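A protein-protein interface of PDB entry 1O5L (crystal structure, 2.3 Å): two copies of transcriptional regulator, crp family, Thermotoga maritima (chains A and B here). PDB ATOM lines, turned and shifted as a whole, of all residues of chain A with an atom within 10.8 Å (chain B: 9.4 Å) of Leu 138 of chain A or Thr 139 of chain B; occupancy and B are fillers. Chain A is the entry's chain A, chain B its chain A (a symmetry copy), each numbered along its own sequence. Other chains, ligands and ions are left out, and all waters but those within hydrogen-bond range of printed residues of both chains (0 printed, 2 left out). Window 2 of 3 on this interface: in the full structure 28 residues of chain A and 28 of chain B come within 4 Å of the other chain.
His 55 of chain A touches Phe 136 of chain B (CD2 to CE1, 3.9 Å).
Val 131 of chain A touches Val 131 of chain B (CG1 to CG1, 3.9 Å).
Val 131 of chain A touches Leu 135 of chain B (CG2 to CD2, 3.3 Å).
Leu 135 of chain B touches Lys 134 of chain A.
Leu 135 of chain A touches Lys 134 of chain B (CD2 to CD, 3.9 Å).
CD1 of Leu 135 of chain B touches CA of Leu 135 of chain A (3.97 Å).
Leu 135 of chain A touches Leu 138 of chain B.
Leu 138 of chain A touches Leu 135 of chain B (CD1 to CD1, 3.96 Å).
Leu 138 of chain A touches Thr 139 of chain B (CD1 to CG2, 3.7 Å).
CG2 of Thr 139 of chain A touches CD1 of Leu 138 of chain B, 3.7 Å away.
Of the printed residues of chain B, His 55 of chain A touches Phe 136.
Glu 64 of chain A touches none of the printed residues of chain B.
Printed residues of chain B within 4 Å of Lys 134 of chain A: Leu 135.
Printed residues of chain B within 4 Å of Leu 135 of chain A: Val 131, Lys 134, Leu 135 and Leu 138.
Of chain B, only Leu 135 (3.96 Å) and Thr 139 (3.7 Å) come within 4 Å of Leu 138 of chain A.
Printed residues of chain B within 4 Å of Thr 139 of chain A: Leu 138.
Lys 141 of chain A touches none of the printed residues of chain B.
Printed residues of chain A within 4 Å of Lys 134 of chain B: Leu 135.
Leu 135 of chain B touches just these residues of chain A: Val 131 (3.3 Å), Lys 134 (3.9 Å), Leu 135 (3.97 Å) and Leu 138 (3.96 Å).
Of the printed residues of chain A, Phe 136 of chain B touches His 55 (3.9 Å).
Leu 138 of chain B touches two residues of chain A.
Thr 140 of chain B touches none of the printed residues of chain A.
No residue of chain A comes within 4 Å of Lys 141 of chain B.
The nearest residue of chain B that does not touch Leu 138 of chain A is Leu 138 of chain B (5.9 Å).
The nearest residue of chain A that does not touch Thr 139 of chain B is Lys 134 of chain A (5.2 Å).
The backbone NH (N) of His 55 of chain A lies within hydrogen-bond range of the backbone carbonyl oxygen (O) of Leu 63 of chain A (2.8 Å).
The backbone carbonyl oxygen (O) of Leu 135 of chain A is in hydrogen-bond range of the side-chain hydroxyl (OG1) of Thr 139 of chain A (2.7 Å).
The side-chain hydroxyl of Thr 139 of chain B lies within hydrogen-bond range of the backbone carbonyl oxygen of Leu 135 of chain B, at 2.7 Å.
The backbone carbonyl oxygen of Phe 136 of chain B sits at hydrogen-bond distance from the side-chain hydroxyl of Thr 140 of chain B, 2.7 Å away.
Hydrophobic or aromatic side chains of chain B within 4 Å of the printed part of chain A: Val 131, Leu 135, Phe 136 and Leu 138.
Of the 18 printed residues of chain A, 6 touch a printed residue of chain B.
Printed residues of chain A that touch a printed residue of chain B: His 55, Val 131, Lys 134, Leu 135, Leu 138 and Thr 139.
Hydrophobic or aromatic side chains of chain A that line the printed part of chain B: His 55, Val 131, Leu 135 and Leu 138.
Among the printed residues, no Asp or Glu carboxylate lies within 4 Å of a Lys or Arg side-chain nitrogen of the other chain.
Val 131 of chain B touches its own counterpart, Val 131 of chain A.
Lys 134 of chain A touches Leu 135 of chain B, and with the chains exchanged Leu 135 of chain A touches Lys 134 of chain B.
Leu 135 of chain B touches its own counterpart, Leu 135 of chain A.
Leu 138 of chain A touches Thr 139 of chain B, and with the chains exchanged Thr 139 of chain A touches Leu 138 of chain B.
Positions printed for both chains: 131, 132, 133, 134, 135, 136, 137, 138, 139, 140 and 141.
Of the 11 pairs that touch across the chains among the printed residues, 10 have their exchanged pair printed and touching as well.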
ATOM      1  N   HIS A  55       9.874 -25.262  13.085  1.00  0.00           N
ATOM      2  CA  HIS A  55       9.446 -23.963  13.594  1.00  0.00           C
ATOM      3  C   HIS A  55       7.946 -23.744  13.394  1.00  0.00           C
ATOM      4  O   HIS A  55       7.413 -23.985  12.319  1.00  0.00           O
ATOM      5  CB  HIS A  55      10.205 -22.839  12.907  1.00  0.00           C
ATOM      6  CG  HIS A  55       9.905 -21.484  13.473  1.00  0.00           C
ATOM      7  ND1 HIS A  55       8.755 -20.782  13.159  1.00  0.00           N
ATOM      8  CD2 HIS A  55      10.592 -20.712  14.350  1.00  0.00           C
ATOM      9  CE1 HIS A  55       8.753 -19.634  13.813  1.00  0.00           C
ATOM     10  NE2 HIS A  55       9.856 -19.566  14.538  1.00  0.00           N
ATOM     11  N   SER A  57       4.764 -21.308  13.263  1.00  0.00           N
ATOM     12  CA  SER A  57       4.455 -19.931  12.917  1.00  0.00           C
ATOM     13  C   SER A  57       3.148 -19.463  13.571  1.00  0.00           C
ATOM     14  O   SER A  57       2.320 -20.248  14.060  1.00  0.00           O
ATOM     15  CB  SER A  57       4.352 -19.768  11.394  1.00  0.00           C
ATOM     16  OG  SER A  57       3.190 -20.414  10.902  1.00  0.00           O
ATOM     17  N   GLU A  58       2.972 -18.158  13.498  1.00  0.00           N
ATOM     18  CA  GLU A  58       1.915 -17.427  14.164  1.00  0.00           C
ATOM     19  C   GLU A  58       0.514 -18.015  13.909  1.00  0.00           C
ATOM     20  O   GLU A  58      -0.417 -17.789  14.697  1.00  0.00           O
ATOM     21  CB  GLU A  58       1.996 -15.945  13.716  1.00  0.00           C
ATOM     22  CG  GLU A  58       3.340 -15.261  14.048  1.00  0.00           C
ATOM     23  CD  GLU A  58       4.531 -15.762  13.206  1.00  0.00           C
ATOM     24  OE1 GLU A  58       4.564 -15.443  11.989  1.00  0.00           O
ATOM     25  OE2 GLU A  58       5.419 -16.492  13.739  1.00  0.00           O
ATOM     26  N   LEU A  63       6.983 -25.495   9.870  1.00  0.00           N
ATOM     27  CA  LEU A  63       8.015 -25.683   8.855  1.00  0.00           C
ATOM     28  C   LEU A  63       9.187 -26.467   9.439  1.00  0.00           C
ATOM     29  O   LEU A  63       9.799 -26.064  10.437  1.00  0.00           O
ATOM     30  CB  LEU A  63       8.482 -24.330   8.298  1.00  0.00           C
ATOM     31  CG  LEU A  63       9.538 -24.317   7.171  1.00  0.00           C
ATOM     32  CD1 LEU A  63       9.047 -25.052   5.933  1.00  0.00           C
ATOM     33  CD2 LEU A  63       9.931 -22.896   6.801  1.00  0.00           C
ATOM     34  N   GLU A  64       9.501 -27.599   8.817  1.00  0.00           N
ATOM     35  CA  GLU A  64      10.674 -28.375   9.229  1.00  0.00           C
ATOM     36  C   GLU A  64      11.958 -27.654   8.832  1.00  0.00           C
ATOM     37  O   GLU A  64      12.073 -27.125   7.743  1.00  0.00           O
ATOM     38  CB  GLU A  64      10.679 -29.795   8.654  1.00  0.00           C
ATOM     39  CG  GLU A  64      11.881 -30.589   9.164  1.00  0.00           C
ATOM     40  CD  GLU A  64      11.909 -32.023   8.726  1.00  0.00           C
ATOM     41  OE1 GLU A  64      10.858 -32.690   8.821  1.00  0.00           O
ATOM     42  OE2 GLU A  64      12.993 -32.469   8.282  1.00  0.00           O
ATOM     43  N   ILE A  65      12.918 -27.687   9.742  1.00  0.00           N
ATOM     44  CA  ILE A  65      14.160 -26.925   9.690  1.00  0.00           C
ATOM     45  C   ILE A  65      15.334 -27.860   9.442  1.00  0.00           C
ATOM     46  O   ILE A  65      16.195 -27.577   8.629  1.00  0.00           O
ATOM     47  CB  ILE A  65      14.341 -26.159  11.068  1.00  0.00           C
ATOM     48  CG1 ILE A  65      13.267 -25.069  11.234  1.00  0.00           C
ATOM     49  CG2 ILE A  65      15.724 -25.532  11.232  1.00  0.00           C
ATOM     50  CD1 ILE A  65      13.048 -24.179  10.012  1.00  0.00           C
ATOM     51  N   VAL A 130      27.985 -20.869  11.811  1.00  0.00           N
ATOM     52  CA  VAL A 130      27.082 -21.183  10.713  1.00  0.00           C
ATOM     53  C   VAL A 130      25.880 -20.198  10.601  1.00  0.00           C
ATOM     54  O   VAL A 130      25.578 -19.720   9.522  1.00  0.00           O
ATOM     55  CB  VAL A 130      26.597 -22.642  10.832  1.00  0.00           C
ATOM     56  CG1 VAL A 130      25.261 -22.840  10.145  1.00  0.00           C
ATOM     57  CG2 VAL A 130      27.648 -23.584  10.254  1.00  0.00           C
ATOM     58  N   VAL A 131      25.231 -19.908  11.724  1.00  0.00           N
ATOM     59  CA  VAL A 131      24.097 -18.989  11.739  1.00  0.00           C
ATOM     60  C   VAL A 131      24.575 -17.531  11.450  1.00  0.00           C
ATOM     61  O   VAL A 131      23.927 -16.773  10.726  1.00  0.00           O
ATOM     62  CB  VAL A 131      23.283 -19.154  13.048  1.00  0.00           C
ATOM     63  CG1 VAL A 131      24.096 -18.828  14.263  1.00  0.00           C
ATOM     64  CG2 VAL A 131      22.105 -18.239  13.073  1.00  0.00           C
ATOM     65  N   SER A 132      25.745 -17.179  11.967  1.00  0.00           N
ATOM     66  CA  SER A 132      26.318 -15.855  11.772  1.00  0.00           C
ATOM     67  C   SER A 132      26.657 -15.552  10.304  1.00  0.00           C
ATOM     68  O   SER A 132      26.350 -14.463   9.805  1.00  0.00           O
ATOM     69  CB  SER A 132      27.540 -15.676  12.678  1.00  0.00           C
ATOM     70  OG  SER A 132      28.197 -14.424  12.442  1.00  0.00           O
ATOM     71  N   GLU A 133      27.275 -16.519   9.632  1.00  0.00           N
ATOM     72  CA  GLU A 133      27.675 -16.413   8.225  1.00  0.00           C
ATOM     73  C   GLU A 133      26.455 -16.368   7.310  1.00  0.00           C
ATOM     74  O   GLU A 133      26.406 -15.571   6.392  1.00  0.00           O
ATOM     75  CB  GLU A 133      28.642 -17.566   7.822  1.00  0.00           C
ATOM     76  CG  GLU A 133      30.071 -17.351   8.355  1.00  0.00           C
ATOM     77  CD  GLU A 133      31.057 -18.484   8.068  1.00  0.00           C
ATOM     78  OE1 GLU A 133      30.740 -19.386   7.275  1.00  0.00           O
ATOM     79  OE2 GLU A 133      32.178 -18.460   8.643  1.00  0.00           O
ATOM     80  N   LYS A 134      25.466 -17.210   7.591  1.00  0.00           N
ATOM     81  CA  LYS A 134      24.187 -17.172   6.895  1.00  0.00           C
ATOM     82  C   LYS A 134      23.513 -15.800   7.034  1.00  0.00           C
ATOM     83  O   LYS A 134      23.052 -15.221   6.041  1.00  0.00           O
ATOM     84  CB  LYS A 134      23.261 -18.286   7.434  1.00  0.00           C
ATOM     85  CG  LYS A 134      21.919 -18.413   6.675  1.00  0.00           C
ATOM     86  CD  LYS A 134      21.140 -19.683   7.023  1.00  0.00           C
ATOM     87  CE  LYS A 134      19.744 -19.667   6.416  1.00  0.00           C
ATOM     88  NZ  LYS A 134      18.872 -20.760   6.893  1.00  0.00           N
ATOM     89  N   LEU A 135      23.458 -15.286   8.268  1.00  0.00           N
ATOM     90  CA  LEU A 135      22.870 -13.979   8.534  1.00  0.00           C
ATOM     91  C   LEU A 135      23.580 -12.849   7.811  1.00  0.00           C
ATOM     92  O   LEU A 135      22.916 -11.940   7.346  1.00  0.00           O
ATOM     93  CB  LEU A 135      22.841 -13.669  10.045  1.00  0.00           C
ATOM     94  CG  LEU A 135      22.124 -12.391  10.508  1.00  0.00           C
ATOM     95  CD1 LEU A 135      20.678 -12.302   9.969  1.00  0.00           C
ATOM     96  CD2 LEU A 135      22.107 -12.315  12.033  1.00  0.00           C
ATOM     97  N   PHE A 136      24.913 -12.883   7.749  1.00  0.00           N
ATOM     98  CA  PHE A 136      25.684 -11.876   6.982  1.00  0.00           C
ATOM     99  C   PHE A 136      25.372 -11.973   5.481  1.00  0.00           C
ATOM    100  O   PHE A 136      25.189 -10.951   4.821  1.00  0.00           O
ATOM    101  CB  PHE A 136      27.210 -12.024   7.165  1.00  0.00           C
ATOM    102  CG  PHE A 136      27.790 -11.249   8.335  1.00  0.00           C
ATOM    103  CD1 PHE A 136      27.657  -9.856   8.424  1.00  0.00           C
ATOM    104  CD2 PHE A 136      28.510 -11.918   9.341  1.00  0.00           C
ATOM    105  CE1 PHE A 136      28.204  -9.145   9.524  1.00  0.00           C
ATOM    106  CE2 PHE A 136      29.070 -11.212  10.448  1.00  0.00           C
ATOM    107  CZ  PHE A 136      28.915  -9.833  10.533  1.00  0.00           C
ATOM    108  N   PHE A 137      25.338 -13.192   4.933  1.00  0.00           N
ATOM    109  CA  PHE A 137      25.103 -13.355   3.485  1.00  0.00           C
ATOM    110  C   PHE A 137      23.720 -12.830   3.074  1.00  0.00           C
ATOM    111  O   PHE A 137      23.559 -12.302   1.997  1.00  0.00           O
ATOM    112  CB  PHE A 137      25.210 -14.807   3.033  1.00  0.00           C
ATOM    113  CG  PHE A 137      26.585 -15.398   3.109  1.00  0.00           C
ATOM    114  CD1 PHE A 137      27.688 -14.742   2.576  1.00  0.00           C
ATOM    115  CD2 PHE A 137      26.754 -16.678   3.612  1.00  0.00           C
ATOM    116  CE1 PHE A 137      28.968 -15.330   2.592  1.00  0.00           C
ATOM    117  CE2 PHE A 137      28.029 -17.282   3.653  1.00  0.00           C
ATOM    118  CZ  PHE A 137      29.135 -16.603   3.130  1.00  0.00           C
ATOM    119  N   LEU A 138      22.732 -12.980   3.939  1.00  0.00           N
ATOM    120  CA  LEU A 138      21.380 -12.497   3.665  1.00  0.00           C
ATOM    121  C   LEU A 138      21.160 -10.983   3.926  1.00  0.00           C
ATOM    122  O   LEU A 138      20.123 -10.463   3.542  1.00  0.00           O
ATOM    123  CB  LEU A 138      20.359 -13.323   4.464  1.00  0.00           C
ATOM    124  CG  LEU A 138      20.237 -14.775   3.975  1.00  0.00           C
ATOM    125  CD1 LEU A 138      19.381 -15.570   4.906  1.00  0.00           C
ATOM    126  CD2 LEU A 138      19.683 -14.852   2.553  1.00  0.00           C
ATOM    127  N   THR A 139      22.118 -10.290   4.555  1.00  0.00           N
ATOM    128  CA  THR A 139      21.970  -8.867   4.876  1.00  0.00           C
ATOM    129  C   THR A 139      23.062  -7.936   4.300  1.00  0.00           C
ATOM    130  O   THR A 139      23.038  -6.739   4.537  1.00  0.00           O
ATOM    131  CB  THR A 139      21.839  -8.675   6.424  1.00  0.00           C
ATOM    132  OG1 THR A 139      22.959  -9.224   7.123  1.00  0.00           O
ATOM    133  CG2 THR A 139      20.676  -9.470   6.980  1.00  0.00           C
ATOM    134  N   THR A 140      24.016  -8.486   3.561  1.00  0.00           N
ATOM    135  CA  THR A 140      25.086  -7.703   2.960  1.00  0.00           C
ATOM    136  C   THR A 140      25.171  -8.033   1.486  1.00  0.00           C
ATOM    137  O   THR A 140      26.244  -8.374   0.970  1.00  0.00           O
ATOM    138  CB  THR A 140      26.444  -8.002   3.583  1.00  0.00           C
ATOM    139  OG1 THR A 140      26.767  -9.385   3.360  1.00  0.00           O
ATOM    140  CG2 THR A 140      26.429  -7.802   5.116  1.00  0.00           C
ATOM    141  N   LYS A 141      24.011  -8.025   0.846  1.00  0.00           N
ATOM    142  CA  LYS A 141      23.859  -7.709  -0.580  1.00  0.00           C
ATOM    143  C   LYS A 141      25.175  -7.606  -1.402  1.00  0.00           C
ATOM    144  O   LYS A 141      25.943  -8.593  -1.433  1.00  0.00           O
ATOM    145  CB  LYS A 141      23.019  -6.425  -0.688  1.00  0.00           C
ATOM    146  CG  LYS A 141      21.992  -6.291   0.476  1.00  0.00           C
ATOM    147  CD  LYS A 141      20.909  -5.248   0.237  1.00  0.00           C
ATOM    148  CE  LYS A 141      19.691  -5.549   1.124  1.00  0.00           C
ATOM    149  NZ  LYS A 141      20.035  -6.160   2.449  1.00  0.00           N
ATOM    150  N   VAL B 131      21.423 -13.698  17.360  1.00  0.00           N
ATOM    151  CA  VAL B 131      21.660 -13.885  15.932  1.00  0.00           C
ATOM    152  C   VAL B 131      20.618 -14.884  15.334  1.00  0.00           C
ATOM    153  O   VAL B 131      20.105 -14.694  14.230  1.00  0.00           O
ATOM    154  CB  VAL B 131      23.141 -14.264  15.672  1.00  0.00           C
ATOM    155  CG1 VAL B 131      23.515 -15.558  16.327  1.00  0.00           C
ATOM    156  CG2 VAL B 131      23.409 -14.436  14.215  1.00  0.00           C
ATOM    157  N   SER B 132      20.267 -15.905  16.106  1.00  0.00           N
ATOM    158  CA  SER B 132      19.302 -16.907  15.683  1.00  0.00           C
ATOM    159  C   SER B 132      17.891 -16.337  15.464  1.00  0.00           C
ATOM    160  O   SER B 132      17.241 -16.646  14.458  1.00  0.00           O
ATOM    161  CB  SER B 132      19.288 -18.072  16.678  1.00  0.00           C
ATOM    162  OG  SER B 132      18.274 -19.034  16.355  1.00  0.00           O
ATOM    163  N   GLU B 133      17.442 -15.507  16.401  1.00  0.00           N
ATOM    164  CA  GLU B 133      16.124 -14.863  16.363  1.00  0.00           C
ATOM    165  C   GLU B 133      16.042 -13.848  15.228  1.00  0.00           C
ATOM    166  O   GLU B 133      15.055 -13.801  14.517  1.00  0.00           O
ATOM    167  CB  GLU B 133      15.770 -14.213  17.733  1.00  0.00           C
ATOM    168  CG  GLU B 133      15.352 -15.250  18.791  1.00  0.00           C
ATOM    169  CD  GLU B 133      15.069 -14.693  20.185  1.00  0.00           C
ATOM    170  OE1 GLU B 133      14.986 -13.464  20.348  1.00  0.00           O
ATOM    171  OE2 GLU B 133      14.918 -15.506  21.135  1.00  0.00           O
ATOM    172  N   LYS B 134      17.099 -13.061  15.055  1.00  0.00           N
ATOM    173  CA  LYS B 134      17.217 -12.152  13.922  1.00  0.00           C
ATOM    174  C   LYS B 134      17.132 -12.905  12.586  1.00  0.00           C
ATOM    175  O   LYS B 134      16.388 -12.500  11.683  1.00  0.00           O
ATOM    176  CB  LYS B 134      18.544 -11.364  14.014  1.00  0.00           C
ATOM    177  CG  LYS B 134      18.711 -10.281  12.925  1.00  0.00           C
ATOM    178  CD  LYS B 134      19.879  -9.327  13.188  1.00  0.00           C
ATOM    179  CE  LYS B 134      20.134  -8.413  11.999  1.00  0.00           C
ATOM    180  NZ  LYS B 134      21.378  -7.622  12.107  1.00  0.00           N
ATOM    181  N   LEU B 135      17.895 -13.995  12.470  1.00  0.00           N
ATOM    182  CA  LEU B 135      17.886 -14.817  11.264  1.00  0.00           C
ATOM    183  C   LEU B 135      16.526 -15.415  10.961  1.00  0.00           C
ATOM    184  O   LEU B 135      16.158 -15.482   9.802  1.00  0.00           O
ATOM    185  CB  LEU B 135      18.929 -15.953  11.347  1.00  0.00           C
ATOM    186  CG  LEU B 135      19.148 -16.825  10.100  1.00  0.00           C
ATOM    187  CD1 LEU B 135      19.453 -15.981   8.841  1.00  0.00           C
ATOM    188  CD2 LEU B 135      20.286 -17.814  10.340  1.00  0.00           C
ATOM    189  N   PHE B 136      15.801 -15.879  11.983  1.00  0.00           N
ATOM    190  CA  PHE B 136      14.425 -16.390  11.794  1.00  0.00           C
ATOM    191  C   PHE B 136      13.482 -15.272  11.323  1.00  0.00           C
ATOM    192  O   PHE B 136      12.674 -15.483  10.420  1.00  0.00           O
ATOM    193  CB  PHE B 136      13.832 -17.003  13.082  1.00  0.00           C
ATOM    194  CG  PHE B 136      14.116 -18.483  13.271  1.00  0.00           C
ATOM    195  CD1 PHE B 136      13.703 -19.432  12.324  1.00  0.00           C
ATOM    196  CD2 PHE B 136      14.770 -18.936  14.431  1.00  0.00           C
ATOM    197  CE1 PHE B 136      13.976 -20.812  12.515  1.00  0.00           C
ATOM    198  CE2 PHE B 136      15.044 -20.322  14.635  1.00  0.00           C
ATOM    199  CZ  PHE B 136      14.646 -21.250  13.681  1.00  0.00           C
ATOM    200  N   PHE B 137      13.565 -14.090  11.944  1.00  0.00           N
ATOM    201  CA  PHE B 137      12.650 -12.990  11.582  1.00  0.00           C
ATOM    202  C   PHE B 137      12.847 -12.547  10.126  1.00  0.00           C
ATOM    203  O   PHE B 137      11.904 -12.175   9.464  1.00  0.00           O
ATOM    204  CB  PHE B 137      12.823 -11.766  12.474  1.00  0.00           C
ATOM    205  CG  PHE B 137      12.401 -11.953  13.901  1.00  0.00           C
ATOM    206  CD1 PHE B 137      11.167 -12.503  14.227  1.00  0.00           C
ATOM    207  CD2 PHE B 137      13.200 -11.462  14.922  1.00  0.00           C
ATOM    208  CE1 PHE B 137      10.749 -12.616  15.568  1.00  0.00           C
ATOM    209  CE2 PHE B 137      12.810 -11.579  16.272  1.00  0.00           C
ATOM    210  CZ  PHE B 137      11.572 -12.151  16.589  1.00  0.00           C
ATOM    211  N   LEU B 138      14.074 -12.592   9.638  1.00  0.00           N
ATOM    212  CA  LEU B 138      14.375 -12.219   8.257  1.00  0.00           C
ATOM    213  C   LEU B 138      14.091 -13.321   7.203  1.00  0.00           C
ATOM    214  O   LEU B 138      14.131 -13.029   6.018  1.00  0.00           O
ATOM    215  CB  LEU B 138      15.837 -11.751   8.150  1.00  0.00           C
ATOM    216  CG  LEU B 138      16.099 -10.414   8.862  1.00  0.00           C
ATOM    217  CD1 LEU B 138      17.562 -10.115   8.887  1.00  0.00           C
ATOM    218  CD2 LEU B 138      15.336  -9.264   8.210  1.00  0.00           C
ATOM    219  N   THR B 139      13.800 -14.559   7.625  1.00  0.00           N
ATOM    220  CA  THR B 139      13.562 -15.666   6.693  1.00  0.00           C
ATOM    221  C   THR B 139      12.192 -16.371   6.833  1.00  0.00           C
ATOM    222  O   THR B 139      11.913 -17.322   6.119  1.00  0.00           O
ATOM    223  CB  THR B 139      14.730 -16.705   6.779  1.00  0.00           C
ATOM    224  OG1 THR B 139      14.898 -17.205   8.107  1.00  0.00           O
ATOM    225  CG2 THR B 139      16.067 -16.051   6.498  1.00  0.00           C
ATOM    226  N   THR B 140      11.354 -15.914   7.753  1.00  0.00           N
ATOM    227  CA  THR B 140      10.035 -16.494   7.964  1.00  0.00           C
ATOM    228  C   THR B 140       9.001 -15.392   7.943  1.00  0.00           C
ATOM    229  O   THR B 140       8.189 -15.262   8.868  1.00  0.00           O
ATOM    230  CB  THR B 140       9.923 -17.212   9.302  1.00  0.00           C
ATOM    231  OG1 THR B 140      10.131 -16.262  10.362  1.00  0.00           O
ATOM    232  CG2 THR B 140      11.017 -18.293   9.469  1.00  0.00           C
ATOM    233  N   LYS B 141       9.112 -14.543   6.931  1.00  0.00           N
ATOM    234  CA  LYS B 141       7.983 -13.814   6.340  1.00  0.00           C
ATOM    235  C   LYS B 141       6.637 -13.892   7.113  1.00  0.00           C
ATOM    236  O   LYS B 141       6.604 -13.505   8.304  1.00  0.00           O
ATOM    237  CB  LYS B 141       7.830 -14.287   4.884  1.00  0.00           C
ATOM    238  CG  LYS B 141       9.194 -14.696   4.251  1.00  0.00           C
ATOM    239  CD  LYS B 141       9.161 -14.830   2.733  1.00  0.00           C
ATOM    240  CE  LYS B 141      10.584 -14.695   2.169  1.00  0.00           C
ATOM    241  NZ  LYS B 141      11.654 -15.237   3.069  1.00  0.00           N
